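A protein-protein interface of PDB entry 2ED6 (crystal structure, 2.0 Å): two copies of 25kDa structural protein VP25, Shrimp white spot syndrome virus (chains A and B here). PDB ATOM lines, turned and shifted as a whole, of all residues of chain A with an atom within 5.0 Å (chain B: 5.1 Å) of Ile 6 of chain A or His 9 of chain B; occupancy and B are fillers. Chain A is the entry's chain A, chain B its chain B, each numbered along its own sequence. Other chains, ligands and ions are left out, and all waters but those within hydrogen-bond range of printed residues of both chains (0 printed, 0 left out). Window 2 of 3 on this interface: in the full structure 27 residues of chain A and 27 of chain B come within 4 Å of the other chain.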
ATOM      1  N   VAL A   2      17.065 -17.753  -0.076  1.00  0.00           N
ATOM      2  CA  VAL A   2      16.233 -18.692  -0.813  1.00  0.00           C
ATOM      3  C   VAL A   2      15.053 -17.956  -1.434  1.00  0.00           C
ATOM      4  O   VAL A   2      14.630 -18.268  -2.546  1.00  0.00           O
ATOM      5  CB  VAL A   2      15.698 -19.799   0.118  1.00  0.00           C
ATOM      6  CG1 VAL A   2      14.778 -20.734  -0.650  1.00  0.00           C
ATOM      7  CG2 VAL A   2      16.860 -20.574   0.720  1.00  0.00           C
ATOM      8  N   THR A   3      14.530 -16.974  -0.707  1.00  0.00           N
ATOM      9  CA  THR A   3      13.398 -16.192  -1.178  1.00  0.00           C
ATOM     10  C   THR A   3      13.675 -15.558  -2.535  1.00  0.00           C
ATOM     11  O   THR A   3      12.857 -15.652  -3.449  1.00  0.00           O
ATOM     12  CB  THR A   3      13.037 -15.074  -0.177  1.00  0.00           C
ATOM     13  OG1 THR A   3      12.643 -15.659   1.070  1.00  0.00           O
ATOM     14  CG2 THR A   3      11.897 -14.220  -0.716  1.00  0.00           C
ATOM     15  N   LYS A   4      14.829 -14.915  -2.668  1.00  0.00           N
ATOM     16  CA  LYS A   4      15.171 -14.263  -3.922  1.00  0.00           C
ATOM     17  C   LYS A   4      15.592 -15.241  -5.015  1.00  0.00           C
ATOM     18  O   LYS A   4      15.486 -14.935  -6.201  1.00  0.00           O
ATOM     19  CB  LYS A   4      16.252 -13.205  -3.688  1.00  0.00           C
ATOM     20  CG  LYS A   4      15.761 -12.067  -2.804  1.00  0.00           C
ATOM     21  CD  LYS A   4      16.630 -10.832  -2.911  1.00  0.00           C
ATOM     22  CE  LYS A   4      16.008  -9.677  -2.138  1.00  0.00           C
ATOM     23  NZ  LYS A   4      16.770  -8.410  -2.304  1.00  0.00           N
ATOM     24  N   THR A   5      16.067 -16.418  -4.620  1.00  0.00           N
ATOM     25  CA  THR A   5      16.461 -17.430  -5.596  1.00  0.00           C
ATOM     26  C   THR A   5      15.191 -17.989  -6.228  1.00  0.00           C
ATOM     27  O   THR A   5      15.140 -18.224  -7.437  1.00  0.00           O
ATOM     28  CB  THR A   5      17.241 -18.582  -4.944  1.00  0.00           C
ATOM     29  OG1 THR A   5      18.521 -18.109  -4.511  1.00  0.00           O
ATOM     30  CG2 THR A   5      17.441 -19.719  -5.937  1.00  0.00           C
ATOM     31  N   ILE A   6      14.172 -18.195  -5.398  1.00  0.00           N
ATOM     32  CA  ILE A   6      12.893 -18.709  -5.865  1.00  0.00           C
ATOM     33  C   ILE A   6      12.243 -17.685  -6.783  1.00  0.00           C
ATOM     34  O   ILE A   6      11.617 -18.049  -7.779  1.00  0.00           O
ATOM     35  CB  ILE A   6      11.951 -19.014  -4.685  1.00  0.00           C
ATOM     36  CG1 ILE A   6      12.515 -20.183  -3.876  1.00  0.00           C
ATOM     37  CG2 ILE A   6      10.553 -19.338  -5.195  1.00  0.00           C
ATOM     38  CD1 ILE A   6      11.661 -20.581  -2.690  1.00  0.00           C
ATOM     39  N   GLU A   7      12.395 -16.408  -6.449  1.00  0.00           N
ATOM     40  CA  GLU A   7      11.828 -15.345  -7.272  1.00  0.00           C
ATOM     41  C   GLU A   7      12.534 -15.351  -8.622  1.00  0.00           C
ATOM     42  O   GLU A   7      11.913 -15.138  -9.661  1.00  0.00           O
ATOM     43  CB  GLU A   7      12.005 -13.983  -6.591  1.00  0.00           C
ATOM     44  CG  GLU A   7      11.220 -13.836  -5.297  1.00  0.00           C
ATOM     45  CD  GLU A   7      11.373 -12.461  -4.673  1.00  0.00           C
ATOM     46  OE1 GLU A   7      11.028 -11.461  -5.338  1.00  0.00           O
ATOM     47  OE2 GLU A   7      11.836 -12.381  -3.516  1.00  0.00           O
ATOM     48  N   THR A   8      13.840 -15.601  -8.600  1.00  0.00           N
ATOM     49  CA  THR A   8      14.620 -15.648  -9.831  1.00  0.00           C
ATOM     50  C   THR A   8      14.150 -16.822 -10.683  1.00  0.00           C
ATOM     51  O   THR A   8      13.949 -16.681 -11.890  1.00  0.00           O
ATOM     52  CB  THR A   8      16.119 -15.800  -9.534  1.00  0.00           C
ATOM     53  OG1 THR A   8      16.578 -14.642  -8.828  1.00  0.00           O
ATOM     54  CG2 THR A   8      16.913 -15.943 -10.824  1.00  0.00           C
ATOM     55  N   HIS A   9      13.973 -17.979 -10.046  1.00  0.00           N
ATOM     56  CA  HIS A   9      13.500 -19.173 -10.735  1.00  0.00           C
ATOM     57  C   HIS A   9      12.143 -18.903 -11.371  1.00  0.00           C
ATOM     58  O   HIS A   9      11.901 -19.290 -12.512  1.00  0.00           O
ATOM     59  CB  HIS A   9      13.387 -20.346  -9.759  1.00  0.00           C
ATOM     60  CG  HIS A   9      14.683 -21.052  -9.507  1.00  0.00           C
ATOM     61  ND1 HIS A   9      15.898 -20.546  -9.913  1.00  0.00           N
ATOM     62  CD2 HIS A   9      14.953 -22.224  -8.886  1.00  0.00           C
ATOM     63  CE1 HIS A   9      16.862 -21.374  -9.551  1.00  0.00           C
ATOM     64  NE2 HIS A   9      16.314 -22.401  -8.927  1.00  0.00           N
ATOM     65  N   THR A  10      11.259 -18.239 -10.632  1.00  0.00           N
ATOM     66  CA  THR A  10       9.935 -17.919 -11.155  1.00  0.00           C
ATOM     67  C   THR A  10      10.065 -17.144 -12.459  1.00  0.00           C
ATOM     68  O   THR A  10       9.386 -17.455 -13.443  1.00  0.00           O
ATOM     69  CB  THR A  10       9.121 -17.086 -10.144  1.00  0.00           C
ATOM     70  OG1 THR A  10       8.876 -17.879  -8.977  1.00  0.00           O
ATOM     71  CG2 THR A  10       7.789 -16.659 -10.750  1.00  0.00           C
ATOM     72  N   ILE A  13      11.705 -19.436 -15.265  1.00  0.00           N
ATOM     73  CA  ILE A  13      10.786 -20.466 -15.728  1.00  0.00           C
ATOM     74  C   ILE A  13       9.815 -19.808 -16.699  1.00  0.00           C
ATOM     75  O   ILE A  13       9.459 -20.375 -17.732  1.00  0.00           O
ATOM     76  CB  ILE A  13      10.006 -21.081 -14.546  1.00  0.00           C
ATOM     77  CG1 ILE A  13      10.942 -21.971 -13.724  1.00  0.00           C
ATOM     78  CG2 ILE A  13       8.807 -21.882 -15.055  1.00  0.00           C
ATOM     79  CD1 ILE A  13      10.324 -22.497 -12.431  1.00  0.00           C
ATOM     80  N   VAL B   2       6.511 -22.273   0.809  1.00  0.00           N
ATOM     81  CA  VAL B   2       7.634 -22.545  -0.080  1.00  0.00           C
ATOM     82  C   VAL B   2       7.521 -23.955  -0.651  1.00  0.00           C
ATOM     83  O   VAL B   2       7.861 -24.199  -1.809  1.00  0.00           O
ATOM     84  CB  VAL B   2       8.972 -22.426   0.669  1.00  0.00           C
ATOM     85  CG1 VAL B   2      10.124 -22.777  -0.253  1.00  0.00           C
ATOM     86  CG2 VAL B   2       9.135 -21.019   1.208  1.00  0.00           C
ATOM     87  N   THR B   5       5.287 -23.950  -3.557  1.00  0.00           N
ATOM     88  CA  THR B   5       5.823 -23.130  -4.639  1.00  0.00           C
ATOM     89  C   THR B   5       6.853 -23.968  -5.392  1.00  0.00           C
ATOM     90  O   THR B   5       6.927 -23.939  -6.623  1.00  0.00           O
ATOM     91  CB  THR B   5       6.506 -21.860  -4.110  1.00  0.00           C
ATOM     92  OG1 THR B   5       5.522 -20.982  -3.546  1.00  0.00           O
ATOM     93  CG2 THR B   5       7.234 -21.144  -5.234  1.00  0.00           C
ATOM     94  N   ILE B   6       7.647 -24.721  -4.636  1.00  0.00           N
ATOM     95  CA  ILE B   6       8.654 -25.589  -5.220  1.00  0.00           C
ATOM     96  C   ILE B   6       7.977 -26.696  -6.026  1.00  0.00           C
ATOM     97  O   ILE B   6       8.481 -27.103  -7.072  1.00  0.00           O
ATOM     98  CB  ILE B   6       9.533 -26.218  -4.136  1.00  0.00           C
ATOM     99  CG1 ILE B   6      10.364 -25.125  -3.465  1.00  0.00           C
ATOM    100  CG2 ILE B   6      10.430 -27.283  -4.741  1.00  0.00           C
ATOM    101  CD1 ILE B   6      11.283 -25.628  -2.382  1.00  0.00           C
ATOM    102  N   GLU B   7       6.841 -27.181  -5.534  1.00  0.00           N
ATOM    103  CA  GLU B   7       6.099 -28.219  -6.234  1.00  0.00           C
ATOM    104  C   GLU B   7       5.584 -27.625  -7.544  1.00  0.00           C
ATOM    105  O   GLU B   7       5.598 -28.281  -8.578  1.00  0.00           O
ATOM    106  CB  GLU B   7       4.930 -28.717  -5.376  1.00  0.00           C
ATOM    107  CG  GLU B   7       5.365 -29.436  -4.103  1.00  0.00           C
ATOM    108  CD  GLU B   7       4.197 -29.981  -3.301  1.00  0.00           C
ATOM    109  OE1 GLU B   7       3.431 -30.803  -3.847  1.00  0.00           O
ATOM    110  OE2 GLU B   7       4.046 -29.588  -2.125  1.00  0.00           O
ATOM    111  N   THR B   8       5.137 -26.376  -7.496  1.00  0.00           N
ATOM    112  CA  THR B   8       4.632 -25.706  -8.689  1.00  0.00           C
ATOM    113  C   THR B   8       5.769 -25.553  -9.703  1.00  0.00           C
ATOM    114  O   THR B   8       5.594 -25.817 -10.890  1.00  0.00           O
ATOM    115  CB  THR B   8       4.059 -24.314  -8.344  1.00  0.00           C
ATOM    116  OG1 THR B   8       2.935 -24.467  -7.466  1.00  0.00           O
ATOM    117  CG2 THR B   8       3.617 -23.587  -9.608  1.00  0.00           C
ATOM    118  N   HIS B   9       6.935 -25.127  -9.223  1.00  0.00           N
ATOM    119  CA  HIS B   9       8.097 -24.968 -10.087  1.00  0.00           C
ATOM    120  C   HIS B   9       8.457 -26.301 -10.733  1.00  0.00           C
ATOM    121  O   HIS B   9       8.769 -26.355 -11.923  1.00  0.00           O
ATOM    122  CB  HIS B   9       9.296 -24.450  -9.296  1.00  0.00           C
ATOM    123  CG  HIS B   9       9.290 -22.967  -9.084  1.00  0.00           C
ATOM    124  ND1 HIS B   9       8.193 -22.179  -9.359  1.00  0.00           N
ATOM    125  CD2 HIS B   9      10.246 -22.131  -8.617  1.00  0.00           C
ATOM    126  CE1 HIS B   9       8.473 -20.921  -9.070  1.00  0.00           C
ATOM    127  NE2 HIS B   9       9.713 -20.864  -8.618  1.00  0.00           N
ATOM    128  N   THR B  10       8.422 -27.374  -9.944  1.00  0.00           N
ATOM    129  CA  THR B  10       8.732 -28.699 -10.472  1.00  0.00           C
ATOM    130  C   THR B  10       7.828 -29.007 -11.663  1.00  0.00           C
ATOM    131  O   THR B  10       8.304 -29.461 -12.707  1.00  0.00           O
ATOM    132  CB  THR B  10       8.545 -29.790  -9.406  1.00  0.00           C
ATOM    133  OG1 THR B  10       9.509 -29.615  -8.366  1.00  0.00           O
ATOM    134  CG2 THR B  10       8.733 -31.177 -10.019  1.00  0.00           C
ATOM    135  N   ASP B  11       6.528 -28.759 -11.509  1.00  0.00           N
ATOM    136  CA  ASP B  11       5.581 -29.005 -12.594  1.00  0.00           C
ATOM    137  C   ASP B  11       5.820 -28.091 -13.797  1.00  0.00           C
ATOM    138  O   ASP B  11       5.784 -28.543 -14.942  1.00  0.00           O
ATOM    139  CB  ASP B  11       4.137 -28.818 -12.125  1.00  0.00           C
ATOM    140  CG  ASP B  11       3.710 -29.853 -11.111  1.00  0.00           C
ATOM    141  OD1 ASP B  11       4.097 -31.034 -11.246  1.00  0.00           O
ATOM    142  OD2 ASP B  11       2.966 -29.483 -10.185  1.00  0.00           O
ATOM    143  N   ASN B  12       6.053 -26.806 -13.540  1.00  0.00           N
ATOM    144  CA  ASN B  12       6.270 -25.854 -14.633  1.00  0.00           C
ATOM    145  C   ASN B  12       7.556 -26.106 -15.402  1.00  0.00           C
ATOM    146  O   ASN B  12       7.607 -25.924 -16.616  1.00  0.00           O
ATOM    147  CB  ASN B  12       6.254 -24.417 -14.108  1.00  0.00           C
ATOM    148  CG  ASN B  12       4.909 -24.026 -13.549  1.00  0.00           C
ATOM    149  OD1 ASN B  12       3.883 -24.594 -13.931  1.00  0.00           O
ATOM    150  ND2 ASN B  12       4.897 -23.045 -12.651  1.00  0.00           N
ATOM    151  N   ILE B  13       8.598 -26.517 -14.691  1.00  0.00           N
ATOM    152  CA  ILE B  13       9.877 -26.810 -15.320  1.00  0.00           C
ATOM    153  C   ILE B  13       9.674 -28.006 -16.235  1.00  0.00           C
ATOM    154  O   ILE B  13      10.211 -28.056 -17.340  1.00  0.00           O
ATOM    155  CB  ILE B  13      10.953 -27.145 -14.261  1.00  0.00           C
ATOM    156  CG1 ILE B  13      11.345 -25.872 -13.510  1.00  0.00           C
ATOM    157  CG2 ILE B  13      12.162 -27.788 -14.919  1.00  0.00           C
ATOM    158  CD1 ILE B  13      12.277 -26.111 -12.341  1.00  0.00           C
ATOM    159  N   GLU B  14       8.886 -28.966 -15.767  1.00  0.00           N
ATOM    160  CA  GLU B  14       8.596 -30.158 -16.545  1.00  0.00           C
ATOM    161  C   GLU B  14       7.833 -29.770 -17.815  1.00  0.00           C
ATOM    162  O   GLU B  14       8.164 -30.230 -18.911  1.00  0.00           O
ATOM    163  CB  GLU B  14       7.772 -31.129 -15.705  1.00  0.00           C
ATOM    164  CG  GLU B  14       7.474 -32.451 -16.388  1.00  0.00           C
ATOM    165  CD  GLU B  14       6.706 -33.390 -15.478  1.00  0.00           C
ATOM    166  OE1 GLU B  14       5.586 -33.030 -15.057  1.00  0.00           O
ATOM    167  OE2 GLU B  14       7.231 -34.478 -15.180  1.00  0.00           O
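The side-chain hydroxyl of Thr 10 of chain A lies close to a ring nitrogen (NE2) of His 9 of chain B (3.1 Å).
Ile 6 of chain A touches just these residues of chain B: Val 2 (3.6 Å), Thr 5 (3.8 Å) and His 9 (3.5 Å).
Of the printed residues of chain B, His 9 of chain A touches His 9.
Of the printed residues of chain A, Ile 13 of chain B touches Ile 13 (3.7 Å).
Printed residues of chain B within 4 Å of Thr 10 of chain A: His 9.
Printed residues of chain A within 4 Å of Thr 5 of chain B: Ile 6 (3.8 Å).
The nearest printed residue of chain A that does not touch His 9 of chain B is Glu 7 of chain A (5.6 Å).
The nearest printed residue of chain B that does not touch Thr 10 of chain A is Thr 5 of chain B (5.2 Å).
Hydrophobic or aromatic side chains of chain A that line the printed part of chain B: Ile 6, His 9 and Ile 13.
Hydrophobic or aromatic side chains of chain B within 4 Å of the printed part of chain A: Val 2, His 9 and Ile 13.
Among the printed residues, 8 pairs touch across the chains.
Ile 6 of chain A touches Val 2 of chain B, but with the chains exchanged Val 2 of chain A does not touch Ile 6 of chain B (6.3 Å).
Ile 6 of chain A touches Thr 5 of chain B, but with the chains exchanged Thr 5 of chain A does not touch Ile 6 of chain B (9.0 Å).
His 9 of chain A touches its own counterpart, His 9 of chain B.
Ile 13 of chain A touches His 9 of chain B, but with the chains exchanged His 9 of chain A does not touch Ile 13 of chain B (5.8 Å).
Positions printed for both chains: 2, 5, 6, 7, 8, 9, 10 and 13.
Of the 8 pairs that touch across the chains among the printed residues, 2 have their exchanged pair printed and touching as well.
Among the printed residues, pairs that only touch across the chains: Ile 6 of chain A with Val 2 of chain B, Ile 6 of chain A with Thr 5 of chain B, Ile 6 of chain A with His 9 of chain B, His 9 of chain A with His 9 of chain B, Ile 13 of chain A with His 9 of chain B, Ile 13 of chain A with Asn 12 of chain B and Ile 13 of chain A with Ile 13 of chain B.
O of Thr 8 of chain B lies close to ND2 of Asn 12 of chain B (3.4 Å).
The side-chain hydroxyl of Thr 10 of chain A sits at hydrogen-bond distance from the backbone carbonyl oxygen of Ile 6 of chain A, at 3.0 Å.
A ring nitrogen (ND1) of His 9 of chain B sits at hydrogen-bond distance from the backbone carbonyl oxygen of Thr 5 of chain B, 3.5 Å away.
The backbone carbonyl oxygen (O) of Thr 5 of chain A lies within hydrogen-bond range of a ring nitrogen (ND1) of His 9 of chain A (3.5 Å).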
